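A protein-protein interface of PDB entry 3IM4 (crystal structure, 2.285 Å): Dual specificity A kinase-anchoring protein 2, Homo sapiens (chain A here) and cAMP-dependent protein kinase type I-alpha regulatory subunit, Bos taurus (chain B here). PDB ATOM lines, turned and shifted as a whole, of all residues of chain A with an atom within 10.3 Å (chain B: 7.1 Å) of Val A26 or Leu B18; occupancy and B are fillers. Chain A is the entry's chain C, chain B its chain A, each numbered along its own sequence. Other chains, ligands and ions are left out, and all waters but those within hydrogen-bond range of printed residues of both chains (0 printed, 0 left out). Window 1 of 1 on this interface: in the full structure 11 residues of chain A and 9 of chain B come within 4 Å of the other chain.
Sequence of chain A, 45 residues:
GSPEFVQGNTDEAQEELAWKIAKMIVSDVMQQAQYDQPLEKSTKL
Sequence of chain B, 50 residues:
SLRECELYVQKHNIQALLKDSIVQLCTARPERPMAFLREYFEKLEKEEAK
The side-chain amino group (NZ) of Lys B19 is in salt-bridge range of the side-chain carboxylate (OE2) of Glu A15, at 3.2 Å.
NZ of Lys B19 lies close to NE1 of Trp A19 (3.0 Å).
The backbone carbonyl oxygen of Glu B6 sits close to the side-chain amide nitrogen of Gln B10.
O of Leu B18 is in hydrogen-bond range of OG of Ser B21, at 2.8 Å.
OD1 of Asp B20 is in salt-bridge range of NZ of Lys B19 (3.6 Å).
Ala A18 touches Lys B19 (CB to O, 3.5 Å).
Ala A18 touches Ile B22 (CB to CG2, 3.7 Å).
CB of Ala A18 touches CG2 of Val B23, at 3.5 Å.
CB of Ala A22 touches CB of Leu B18 (3.8 Å).
Ile B22 touches Ala A22 (CD1 to N, 3.8 Å).
Lys A23 touches Gln B15 (CG to OE1, 3.6 Å).
Val A26 touches Gln B15 (CG2 to OE1, 3.6 Å).
Val A26 touches Leu B18 (CG2 to CD1, 3.98 Å).
CE of Met A30 touches SG of Cys B5, at 3.4 Å.
CG of Met A30 touches OE2 of Glu B6, at 3.9 Å.
Of the printed residues of chain B, Val A26 touches Gln B15 (3.6 Å) and Leu B18 (3.98 Å).
Of the printed residues of chain A, Leu B18 touches Ala A22 (3.8 Å) and Val A26 (3.98 Å).
Gln B15 touches four residues of chain A.
Printed residues of chain A within 4 Å of Ala B16: Trp A19.
No residue of chain A comes within 4 Å of Leu B17.
Of the printed residues of chain A, Lys B19 touches Glu A15, Ala A18, Trp A19 and Ala A22.
Of the printed residues of chain B, Ala A22 touches Gln B15, Leu B18, Lys B19 and Ile B22.
Of the printed residues of chain A, Glu B6 touches Met A30.
Printed residues of chain B within 4 Å of Glu A15: Lys B19.
Ser A27 touches none of the printed residues of chain B.
Gln B10 touches none of the printed residues of chain A.
The nearest printed residue of chain B that does not touch Val A26 is Val B9 (4.7 Å).
The nearest printed residue of chain A that does not touch Leu B18 is Ile A25 (4.04 Å).
Hydrophobic or aromatic side chains of chain B that line the printed part of chain A: Ala B16, Leu B18, Ile B22 and Val B23.
Printed residues of chain A that touch a printed residue of chain B: Glu A15, Ala A18, Trp A19, Ile A21, Ala A22, Lys A23, Ile A25, Val A26 and Met A30.
Hydrophobic or aromatic side chains of chain A within 4 Å of the printed part of chain B: Ala A18, Trp A19, Ile A21, Ala A22, Ile A25, Val A26 and Met A30.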
ATOM      1  N   GLN A  14     -30.866  -7.058   7.223  1.00  0.00           N
ATOM      2  CA  GLN A  14     -29.443  -7.186   6.911  1.00  0.00           C
ATOM      3  C   GLN A  14     -28.807  -8.309   7.716  1.00  0.00           C
ATOM      4  O   GLN A  14     -28.243  -9.240   7.152  1.00  0.00           O
ATOM      5  CB  GLN A  14     -28.706  -5.871   7.167  1.00  0.00           C
ATOM      6  N   GLU A  15     -28.907  -8.214   9.037  1.00  0.00           N
ATOM      7  CA  GLU A  15     -28.266  -9.170   9.932  1.00  0.00           C
ATOM      8  C   GLU A  15     -28.747 -10.600   9.688  1.00  0.00           C
ATOM      9  O   GLU A  15     -27.961 -11.550   9.750  1.00  0.00           O
ATOM     10  CB  GLU A  15     -28.483  -8.775  11.396  1.00  0.00           C
ATOM     11  CG  GLU A  15     -27.781  -9.699  12.385  1.00  0.00           C
ATOM     12  CD  GLU A  15     -27.958  -9.267  13.829  1.00  0.00           C
ATOM     13  OE1 GLU A  15     -28.494  -8.160  14.056  1.00  0.00           O
ATOM     14  OE2 GLU A  15     -27.562 -10.035  14.736  1.00  0.00           O
ATOM     15  N   LEU A  17     -29.687 -11.728   6.851  1.00  0.00           N
ATOM     16  CA  LEU A  17     -29.044 -12.117   5.604  1.00  0.00           C
ATOM     17  C   LEU A  17     -27.567 -12.441   5.819  1.00  0.00           C
ATOM     18  O   LEU A  17     -27.026 -13.370   5.219  1.00  0.00           O
ATOM     19  CB  LEU A  17     -29.179 -10.995   4.578  1.00  0.00           C
ATOM     20  CG  LEU A  17     -28.348 -11.212   3.315  1.00  0.00           C
ATOM     21  CD1 LEU A  17     -28.798 -12.477   2.603  1.00  0.00           C
ATOM     22  CD2 LEU A  17     -28.444 -10.012   2.401  1.00  0.00           C
ATOM     23  N   ALA A  18     -26.914 -11.660   6.669  1.00  0.00           N
ATOM     24  CA  ALA A  18     -25.513 -11.907   7.000  1.00  0.00           C
ATOM     25  C   ALA A  18     -25.344 -13.276   7.662  1.00  0.00           C
ATOM     26  O   ALA A  18     -24.389 -13.997   7.375  1.00  0.00           O
ATOM     27  CB  ALA A  18     -24.967 -10.793   7.893  1.00  0.00           C
ATOM     28  N   TRP A  19     -26.279 -13.639   8.535  1.00  0.00           N
ATOM     29  CA  TRP A  19     -26.249 -14.958   9.168  1.00  0.00           C
ATOM     30  C   TRP A  19     -26.362 -16.073   8.142  1.00  0.00           C
ATOM     31  O   TRP A  19     -25.592 -17.036   8.173  1.00  0.00           O
ATOM     32  CB  TRP A  19     -27.349 -15.102  10.224  1.00  0.00           C
ATOM     33  CG  TRP A  19     -26.929 -14.591  11.568  1.00  0.00           C
ATOM     34  CD1 TRP A  19     -27.484 -13.554  12.270  1.00  0.00           C
ATOM     35  CD2 TRP A  19     -25.838 -15.080  12.366  1.00  0.00           C
ATOM     36  NE1 TRP A  19     -26.812 -13.376  13.460  1.00  0.00           N
ATOM     37  CE2 TRP A  19     -25.799 -14.297  13.543  1.00  0.00           C
ATOM     38  CE3 TRP A  19     -24.900 -16.105  12.203  1.00  0.00           C
ATOM     39  CZ2 TRP A  19     -24.854 -14.511  14.553  1.00  0.00           C
ATOM     40  CZ3 TRP A  19     -23.964 -16.318  13.207  1.00  0.00           C
ATOM     41  CH2 TRP A  19     -23.950 -15.523  14.367  1.00  0.00           C
ATOM     42  N   LYS A  20     -27.324 -15.932   7.234  1.00  0.00           N
ATOM     43  CA  LYS A  20     -27.531 -16.916   6.180  1.00  0.00           C
ATOM     44  C   LYS A  20     -26.241 -17.109   5.408  1.00  0.00           C
ATOM     45  O   LYS A  20     -25.743 -18.228   5.275  1.00  0.00           O
ATOM     46  CB  LYS A  20     -28.630 -16.462   5.224  1.00  0.00           C
ATOM     47  CG  LYS A  20     -28.959 -17.489   4.152  1.00  0.00           C
ATOM     48  CD  LYS A  20     -29.126 -16.835   2.787  1.00  0.00           C
ATOM     49  CE  LYS A  20     -30.394 -16.004   2.701  1.00  0.00           C
ATOM     50  NZ  LYS A  20     -31.587 -16.852   2.447  1.00  0.00           N
ATOM     51  N   ILE A  21     -25.693 -16.012   4.901  1.00  0.00           N
ATOM     52  CA  ILE A  21     -24.438 -16.086   4.159  1.00  0.00           C
ATOM     53  C   ILE A  21     -23.284 -16.677   4.984  1.00  0.00           C
ATOM     54  O   ILE A  21     -22.521 -17.491   4.479  1.00  0.00           O
ATOM     55  CB  ILE A  21     -24.051 -14.726   3.571  1.00  0.00           C
ATOM     56  CG1 ILE A  21     -25.091 -14.312   2.531  1.00  0.00           C
ATOM     57  CG2 ILE A  21     -22.670 -14.791   2.938  1.00  0.00           C
ATOM     58  CD1 ILE A  21     -25.014 -12.856   2.130  1.00  0.00           C
ATOM     59  N   ALA A  22     -23.166 -16.286   6.249  1.00  0.00           N
ATOM     60  CA  ALA A  22     -22.092 -16.815   7.095  1.00  0.00           C
ATOM     61  C   ALA A  22     -22.212 -18.327   7.292  1.00  0.00           C
ATOM     62  O   ALA A  22     -21.212 -19.039   7.250  1.00  0.00           O
ATOM     63  CB  ALA A  22     -22.053 -16.104   8.445  1.00  0.00           C
ATOM     64  N   LYS A  23     -23.430 -18.815   7.514  1.00  0.00           N
ATOM     65  CA  LYS A  23     -23.656 -20.255   7.650  1.00  0.00           C
ATOM     66  C   LYS A  23     -23.332 -20.995   6.350  1.00  0.00           C
ATOM     67  O   LYS A  23     -22.890 -22.141   6.376  1.00  0.00           O
ATOM     68  CB  LYS A  23     -25.092 -20.556   8.095  1.00  0.00           C
ATOM     69  CG  LYS A  23     -25.435 -20.069   9.502  1.00  0.00           C
ATOM     70  CD  LYS A  23     -26.858 -20.467   9.912  1.00  0.00           C
ATOM     71  CE  LYS A  23     -26.988 -21.978  10.084  1.00  0.00           C
ATOM     72  NZ  LYS A  23     -28.375 -22.403  10.433  1.00  0.00           N
ATOM     73  N   MET A  24     -23.554 -20.330   5.220  1.00  0.00           N
ATOM     74  CA  MET A  24     -23.188 -20.872   3.914  1.00  0.00           C
ATOM     75  C   MET A  24     -21.682 -21.053   3.821  1.00  0.00           C
ATOM     76  O   MET A  24     -21.193 -22.106   3.421  1.00  0.00           O
ATOM     77  CB  MET A  24     -23.644 -19.936   2.792  1.00  0.00           C
ATOM     78  CG  MET A  24     -25.150 -19.864   2.587  1.00  0.00           C
ATOM     79  SD  MET A  24     -25.560 -19.236   0.943  1.00  0.00           S
ATOM     80  CE  MET A  24     -24.703 -20.430  -0.087  1.00  0.00           C
ATOM     81  N   ILE A  25     -20.947 -20.010   4.185  1.00  0.00           N
ATOM     82  CA  ILE A  25     -19.495 -20.066   4.161  1.00  0.00           C
ATOM     83  C   ILE A  25     -18.975 -21.160   5.092  1.00  0.00           C
ATOM     84  O   ILE A  25     -18.039 -21.875   4.748  1.00  0.00           O
ATOM     85  CB  ILE A  25     -18.877 -18.718   4.561  1.00  0.00           C
ATOM     86  CG1 ILE A  25     -19.382 -17.606   3.638  1.00  0.00           C
ATOM     87  CG2 ILE A  25     -17.363 -18.807   4.532  1.00  0.00           C
ATOM     88  CD1 ILE A  25     -18.920 -16.214   4.040  1.00  0.00           C
ATOM     89  N   VAL A  26     -19.583 -21.292   6.269  1.00  0.00           N
ATOM     90  CA  VAL A  26     -19.130 -22.286   7.239  1.00  0.00           C
ATOM     91  C   VAL A  26     -19.303 -23.700   6.682  1.00  0.00           C
ATOM     92  O   VAL A  26     -18.448 -24.559   6.885  1.00  0.00           O
ATOM     93  CB  VAL A  26     -19.858 -22.150   8.588  1.00  0.00           C
ATOM     94  CG1 VAL A  26     -19.697 -23.417   9.402  1.00  0.00           C
ATOM     95  CG2 VAL A  26     -19.338 -20.944   9.360  1.00  0.00           C
ATOM     96  N   SER A  27     -20.408 -23.931   5.979  1.00  0.00           N
ATOM     97  CA  SER A  27     -20.633 -25.195   5.282  1.00  0.00           C
ATOM     98  C   SER A  27     -19.536 -25.491   4.272  1.00  0.00           C
ATOM     99  O   SER A  27     -18.885 -26.530   4.338  1.00  0.00           O
ATOM    100  CB  SER A  27     -21.984 -25.190   4.568  1.00  0.00           C
ATOM    101  OG  SER A  27     -22.919 -26.011   5.249  1.00  0.00           O
ATOM    102  N   ASP A  28     -19.337 -24.571   3.337  1.00  0.00           N
ATOM    103  CA  ASP A  28     -18.315 -24.732   2.311  1.00  0.00           C
ATOM    104  C   ASP A  28     -16.930 -24.907   2.930  1.00  0.00           C
ATOM    105  O   ASP A  28     -16.081 -25.604   2.374  1.00  0.00           O
ATOM    106  CB  ASP A  28     -18.330 -23.543   1.352  1.00  0.00           C
ATOM    107  CG  ASP A  28     -19.736 -23.163   0.916  1.00  0.00           C
ATOM    108  OD1 ASP A  28     -20.658 -23.995   1.061  1.00  0.00           O
ATOM    109  OD2 ASP A  28     -19.921 -22.026   0.432  1.00  0.00           O
ATOM    110  N   VAL A  29     -16.701 -24.285   4.084  1.00  0.00           N
ATOM    111  CA  VAL A  29     -15.424 -24.459   4.769  1.00  0.00           C
ATOM    112  C   VAL A  29     -15.269 -25.886   5.301  1.00  0.00           C
ATOM    113  O   VAL A  29     -14.229 -26.508   5.102  1.00  0.00           O
ATOM    114  CB  VAL A  29     -15.206 -23.432   5.905  1.00  0.00           C
ATOM    115  CG1 VAL A  29     -14.032 -23.850   6.785  1.00  0.00           C
ATOM    116  CG2 VAL A  29     -14.975 -22.032   5.328  1.00  0.00           C
ATOM    117  N   MET A  30     -16.299 -26.405   5.964  1.00  0.00           N
ATOM    118  CA  MET A  30     -16.254 -27.785   6.446  1.00  0.00           C
ATOM    119  C   MET A  30     -16.052 -28.778   5.296  1.00  0.00           C
ATOM    120  O   MET A  30     -15.303 -29.745   5.423  1.00  0.00           O
ATOM    121  CB  MET A  30     -17.518 -28.148   7.236  1.00  0.00           C
ATOM    122  CG  MET A  30     -17.640 -27.498   8.613  1.00  0.00           C
ATOM    123  SD  MET A  30     -16.078 -27.378   9.510  1.00  0.00           S
ATOM    124  CE  MET A  30     -15.605 -25.687   9.163  1.00  0.00           C
ATOM    125  N   GLN A  31     -16.727 -28.535   4.176  1.00  0.00           N
ATOM    126  CA  GLN A  31     -16.603 -29.396   3.006  1.00  0.00           C
ATOM    127  C   GLN A  31     -15.161 -29.429   2.502  1.00  0.00           C
ATOM    128  O   GLN A  31     -14.568 -30.497   2.360  1.00  0.00           O
ATOM    129  CB  GLN A  31     -17.546 -28.932   1.904  1.00  0.00           C
ATOM    130  N   GLN A  32     -14.603 -28.251   2.240  1.00  0.00           N
ATOM    131  CA  GLN A  32     -13.226 -28.131   1.773  1.00  0.00           C
ATOM    132  C   GLN A  32     -12.224 -28.717   2.770  1.00  0.00           C
ATOM    133  O   GLN A  32     -11.086 -29.018   2.410  1.00  0.00           O
ATOM    134  CB  GLN A  32     -12.891 -26.664   1.495  1.00  0.00           C
ATOM    135  CG  GLN A  32     -11.493 -26.427   0.937  1.00  0.00           C
ATOM    136  CD  GLN A  32     -11.342 -26.895  -0.501  1.00  0.00           C
ATOM    137  OE1 GLN A  32     -12.309 -26.922  -1.265  1.00  0.00           O
ATOM    138  NE2 GLN A  32     -10.121 -27.263  -0.877  1.00  0.00           N
ATOM    139  N   ALA A  33     -12.651 -28.881   4.020  1.00  0.00           N
ATOM    140  CA  ALA A  33     -11.782 -29.408   5.070  1.00  0.00           C
ATOM    141  C   ALA A  33     -11.847 -30.930   5.157  1.00  0.00           C
ATOM    142  O   ALA A  33     -11.016 -31.557   5.816  1.00  0.00           O
ATOM    143  CB  ALA A  33     -12.126 -28.780   6.421  1.00  0.00           C
ATOM    144  N   GLN A  34     -12.846 -31.514   4.505  1.00  0.00           N
ATOM    145  CA  GLN A  34     -12.935 -32.961   4.383  1.00  0.00           C
ATOM    146  C   GLN A  34     -12.152 -33.414   3.154  1.00  0.00           C
ATOM    147  O   GLN A  34     -11.600 -34.512   3.132  1.00  0.00           O
ATOM    148  CB  GLN A  34     -14.388 -33.404   4.289  1.00  0.00           C
ATOM    149  N   CYS B   5     -11.021 -28.483  12.834  1.00  0.00           N
ATOM    150  CA  CYS B   5     -11.529 -27.256  12.233  1.00  0.00           C
ATOM    151  C   CYS B   5     -12.915 -26.914  12.766  1.00  0.00           C
ATOM    152  O   CYS B   5     -13.201 -25.765  13.089  1.00  0.00           O
ATOM    153  CB  CYS B   5     -11.580 -27.382  10.707  1.00  0.00           C
ATOM    154  SG  CYS B   5     -12.234 -25.917   9.852  1.00  0.00           S
ATOM    155  N   GLU B   6     -13.774 -27.919  12.854  1.00  0.00           N
ATOM    156  CA  GLU B   6     -15.117 -27.723  13.373  1.00  0.00           C
ATOM    157  C   GLU B   6     -15.017 -27.207  14.800  1.00  0.00           C
ATOM    158  O   GLU B   6     -15.672 -26.239  15.175  1.00  0.00           O
ATOM    159  CB  GLU B   6     -15.883 -29.043  13.341  1.00  0.00           C
ATOM    160  CG  GLU B   6     -17.332 -28.924  12.921  1.00  0.00           C
ATOM    161  CD  GLU B   6     -17.872 -30.227  12.348  1.00  0.00           C
ATOM    162  OE1 GLU B   6     -17.621 -31.295  12.950  1.00  0.00           O
ATOM    163  OE2 GLU B   6     -18.546 -30.181  11.295  1.00  0.00           O
ATOM    164  N   VAL B   9     -13.810 -23.538  14.969  1.00  0.00           N
ATOM    165  CA  VAL B   9     -14.852 -22.619  14.565  1.00  0.00           C
ATOM    166  C   VAL B   9     -15.815 -22.354  15.714  1.00  0.00           C
ATOM    167  O   VAL B   9     -16.152 -21.202  15.993  1.00  0.00           O
ATOM    168  CB  VAL B   9     -15.607 -23.168  13.357  1.00  0.00           C
ATOM    169  CG1 VAL B   9     -16.889 -22.384  13.132  1.00  0.00           C
ATOM    170  CG2 VAL B   9     -14.704 -23.122  12.134  1.00  0.00           C
ATOM    171  N   GLN B  10     -16.240 -23.423  16.386  1.00  0.00           N
ATOM    172  CA  GLN B  10     -17.159 -23.302  17.516  1.00  0.00           C
ATOM    173  C   GLN B  10     -16.546 -22.523  18.677  1.00  0.00           C
ATOM    174  O   GLN B  10     -17.120 -21.547  19.160  1.00  0.00           O
ATOM    175  CB  GLN B  10     -17.609 -24.683  18.010  1.00  0.00           C
ATOM    176  CG  GLN B  10     -18.190 -25.577  16.928  1.00  0.00           C
ATOM    177  CD  GLN B  10     -19.091 -24.827  15.966  1.00  0.00           C
ATOM    178  OE1 GLN B  10     -20.186 -24.391  16.330  1.00  0.00           O
ATOM    179  NE2 GLN B  10     -18.636 -24.679  14.725  1.00  0.00           N
ATOM    180  N   ASN B  13     -16.071 -18.728  18.031  1.00  0.00           N
ATOM    181  CA  ASN B  13     -17.190 -18.022  17.404  1.00  0.00           C
ATOM    182  C   ASN B  13     -16.887 -17.477  16.010  1.00  0.00           C
ATOM    183  O   ASN B  13     -17.274 -16.362  15.675  1.00  0.00           O
ATOM    184  CB  ASN B  13     -17.655 -16.876  18.303  1.00  0.00           C
ATOM    185  CG  ASN B  13     -18.065 -17.351  19.680  1.00  0.00           C
ATOM    186  OD1 ASN B  13     -18.672 -18.415  19.831  1.00  0.00           O
ATOM    187  ND2 ASN B  13     -17.733 -16.565  20.699  1.00  0.00           N
ATOM    188  N   ILE B  14     -16.197 -18.268  15.197  1.00  0.00           N
ATOM    189  CA  ILE B  14     -15.884 -17.855  13.840  1.00  0.00           C
ATOM    190  C   ILE B  14     -17.130 -17.556  13.006  1.00  0.00           C
ATOM    191  O   ILE B  14     -17.114 -16.661  12.167  1.00  0.00           O
ATOM    192  CB  ILE B  14     -14.998 -18.886  13.116  1.00  0.00           C
ATOM    193  CG1 ILE B  14     -13.664 -19.032  13.851  1.00  0.00           C
ATOM    194  CG2 ILE B  14     -14.763 -18.467  11.672  1.00  0.00           C
ATOM    195  CD1 ILE B  14     -13.049 -17.707  14.246  1.00  0.00           C
ATOM    196  N   GLN B  15     -18.210 -18.294  13.229  1.00  0.00           N
ATOM    197  CA  GLN B  15     -19.424 -18.054  12.451  1.00  0.00           C
ATOM    198  C   GLN B  15     -19.988 -16.652  12.686  1.00  0.00           C
ATOM    199  O   GLN B  15     -20.379 -15.968  11.737  1.00  0.00           O
ATOM    200  CB  GLN B  15     -20.496 -19.107  12.733  1.00  0.00           C
ATOM    201  CG  GLN B  15     -21.613 -19.092  11.702  1.00  0.00           C
ATOM    202  CD  GLN B  15     -22.558 -20.269  11.836  1.00  0.00           C
ATOM    203  OE1 GLN B  15     -22.416 -21.282  11.145  1.00  0.00           O
ATOM    204  NE2 GLN B  15     -23.532 -20.143  12.728  1.00  0.00           N
ATOM    205  N   ALA B  16     -20.026 -16.234  13.951  1.00  0.00           N
ATOM    206  CA  ALA B  16     -20.503 -14.903  14.312  1.00  0.00           C
ATOM    207  C   ALA B  16     -19.534 -13.824  13.811  1.00  0.00           C
ATOM    208  O   ALA B  16     -19.940 -12.731  13.404  1.00  0.00           O
ATOM    209  CB  ALA B  16     -20.713 -14.800  15.820  1.00  0.00           C
ATOM    210  N   LEU B  17     -18.250 -14.151  13.819  1.00  0.00           N
ATOM    211  CA  LEU B  17     -17.233 -13.265  13.265  1.00  0.00           C
ATOM    212  C   LEU B  17     -17.487 -12.979  11.776  1.00  0.00           C
ATOM    213  O   LEU B  17     -17.405 -11.831  11.331  1.00  0.00           O
ATOM    214  CB  LEU B  17     -15.856 -13.887  13.479  1.00  0.00           C
ATOM    215  CG  LEU B  17     -14.596 -13.252  12.901  1.00  0.00           C
ATOM    216  CD1 LEU B  17     -13.402 -13.966  13.483  1.00  0.00           C
ATOM    217  CD2 LEU B  17     -14.573 -13.380  11.389  1.00  0.00           C
ATOM    218  N   LEU B  18     -17.794 -14.021  11.012  1.00  0.00           N
ATOM    219  CA  LEU B  18     -18.150 -13.860   9.603  1.00  0.00           C
ATOM    220  C   LEU B  18     -19.391 -13.018   9.447  1.00  0.00           C
ATOM    221  O   LEU B  18     -19.458 -12.160   8.573  1.00  0.00           O
ATOM    222  CB  LEU B  18     -18.430 -15.212   8.955  1.00  0.00           C
ATOM    223  CG  LEU B  18     -17.219 -16.048   8.557  1.00  0.00           C
ATOM    224  CD1 LEU B  18     -17.670 -17.474   8.335  1.00  0.00           C
ATOM    225  CD2 LEU B  18     -16.590 -15.468   7.301  1.00  0.00           C
ATOM    226  N   LYS B  19     -20.391 -13.299  10.278  1.00  0.00           N
ATOM    227  CA  LYS B  19     -21.646 -12.581  10.213  1.00  0.00           C
ATOM    228  C   LYS B  19     -21.390 -11.075  10.366  1.00  0.00           C
ATOM    229  O   LYS B  19     -21.889 -10.268   9.578  1.00  0.00           O
ATOM    230  CB  LYS B  19     -22.611 -13.094  11.286  1.00  0.00           C
ATOM    231  CG  LYS B  19     -24.051 -12.651  11.117  1.00  0.00           C
ATOM    232  CD  LYS B  19     -24.234 -11.164  11.354  1.00  0.00           C
ATOM    233  CE  LYS B  19     -23.813 -10.757  12.753  1.00  0.00           C
ATOM    234  NZ  LYS B  19     -24.737 -11.271  13.796  1.00  0.00           N
ATOM    235  N   ASP B  20     -20.608 -10.703  11.375  1.00  0.00           N
ATOM    236  CA  ASP B  20     -20.325  -9.293  11.635  1.00  0.00           C
ATOM    237  C   ASP B  20     -19.562  -8.680  10.470  1.00  0.00           C
ATOM    238  O   ASP B  20     -19.808  -7.539  10.098  1.00  0.00           O
ATOM    239  CB  ASP B  20     -19.521  -9.117  12.927  1.00  0.00           C
ATOM    240  CG  ASP B  20     -20.321  -9.479  14.172  1.00  0.00           C
ATOM    241  OD1 ASP B  20     -21.545  -9.685  14.051  1.00  0.00           O
ATOM    242  OD2 ASP B  20     -19.726  -9.556  15.275  1.00  0.00           O
ATOM    243  N   SER B  21     -18.640  -9.440   9.889  1.00  0.00           N
ATOM    244  CA  SER B  21     -17.826  -8.920   8.800  1.00  0.00           C
ATOM    245  C   SER B  21     -18.681  -8.709   7.554  1.00  0.00           C
ATOM    246  O   SER B  21     -18.479  -7.747   6.818  1.00  0.00           O
ATOM    247  CB  SER B  21     -16.652  -9.844   8.496  1.00  0.00           C
ATOM    248  OG  SER B  21     -17.090 -10.979   7.783  1.00  0.00           O
ATOM    249  N   ILE B  22     -19.650  -9.595   7.333  1.00  0.00           N
ATOM    250  CA  ILE B  22     -20.554  -9.462   6.194  1.00  0.00           C
ATOM    251  C   ILE B  22     -21.498  -8.275   6.393  1.00  0.00           C
ATOM    252  O   ILE B  22     -21.758  -7.518   5.463  1.00  0.00           O
ATOM    253  CB  ILE B  22     -21.371 -10.735   5.975  1.00  0.00           C
ATOM    254  CG1 ILE B  22     -20.503 -11.820   5.350  1.00  0.00           C
ATOM    255  CG2 ILE B  22     -22.578 -10.470   5.090  1.00  0.00           C
ATOM    256  CD1 ILE B  22     -20.996 -13.213   5.665  1.00  0.00           C
ATOM    257  N   VAL B  23     -22.011  -8.119   7.608  1.00  0.00           N
ATOM    258  CA  VAL B  23     -22.830  -6.961   7.940  1.00  0.00           C
ATOM    259  C   VAL B  23     -22.094  -5.676   7.582  1.00  0.00           C
ATOM    260  O   VAL B  23     -22.664  -4.774   6.969  1.00  0.00           O
ATOM    261  CB  VAL B  23     -23.178  -6.914   9.446  1.00  0.00           C
ATOM    262  CG1 VAL B  23     -23.539  -5.493   9.867  1.00  0.00           C
ATOM    263  CG2 VAL B  23     -24.310  -7.868   9.764  1.00  0.00           C
ATOM    264  N   GLN B  24     -20.826  -5.597   7.975  1.00  0.00           N
ATOM    265  CA  GLN B  24     -20.019  -4.414   7.695  1.00  0.00           C
ATOM    266  C   GLN B  24     -19.861  -4.244   6.198  1.00  0.00           C
ATOM    267  O   GLN B  24     -20.087  -3.168   5.655  1.00  0.00           O
ATOM    268  CB  GLN B  24     -18.646  -4.530   8.355  1.00  0.00           C
ATOM    269  CG  GLN B  24     -18.693  -4.324   9.852  1.00  0.00           C
ATOM    270  CD  GLN B  24     -19.346  -3.009  10.198  1.00  0.00           C
ATOM    271  OE1 GLN B  24     -20.533  -2.959  10.522  1.00  0.00           O
ATOM    272  NE2 GLN B  24     -18.580  -1.923  10.091  1.00  0.00           N
ATOM    273  N   TYR B  40     -10.841  -3.674   8.851  1.00  0.00           N
ATOM    274  CA  TYR B  40     -11.843  -4.126   9.790  1.00  0.00           C
ATOM    275  C   TYR B  40     -11.211  -5.047  10.835  1.00  0.00           C
ATOM    276  O   TYR B  40     -11.425  -4.870  12.032  1.00  0.00           O
ATOM    277  CB  TYR B  40     -12.964  -4.833   9.031  1.00  0.00           C
ATOM    278  CG  TYR B  40     -13.948  -5.576   9.893  1.00  0.00           C
ATOM    279  CD1 TYR B  40     -14.935  -4.898  10.585  1.00  0.00           C
ATOM    280  CD2 TYR B  40     -13.908  -6.960   9.997  1.00  0.00           C
ATOM    281  CE1 TYR B  40     -15.842  -5.567  11.370  1.00  0.00           C
ATOM    282  CE2 TYR B  40     -14.815  -7.638  10.777  1.00  0.00           C
ATOM    283  CZ  TYR B  40     -15.785  -6.930  11.460  1.00  0.00           C
ATOM    284  OH  TYR B  40     -16.703  -7.578  12.246  1.00  0.00           O
ATOM    285  N   PHE B  41     -10.424  -6.023  10.383  1.00  0.00           N
ATOM    286  CA  PHE B  41      -9.762  -6.937  11.317  1.00  0.00           C
ATOM    287  C   PHE B  41      -8.640  -6.271  12.079  1.00  0.00           C
ATOM    288  O   PHE B  41      -8.449  -6.543  13.262  1.00  0.00           O
ATOM    289  CB  PHE B  41      -9.294  -8.228  10.633  1.00  0.00           C
ATOM    290  CG  PHE B  41     -10.428  -9.102  10.216  1.00  0.00           C
ATOM    291  CD1 PHE B  41     -11.252  -9.676  11.170  1.00  0.00           C
ATOM    292  CD2 PHE B  41     -10.713  -9.304   8.877  1.00  0.00           C
ATOM    293  CE1 PHE B  41     -12.328 -10.465  10.796  1.00  0.00           C
ATOM    294  CE2 PHE B  41     -11.781 -10.090   8.496  1.00  0.00           C
ATOM    295  CZ  PHE B  41     -12.591 -10.676   9.459  1.00  0.00           C
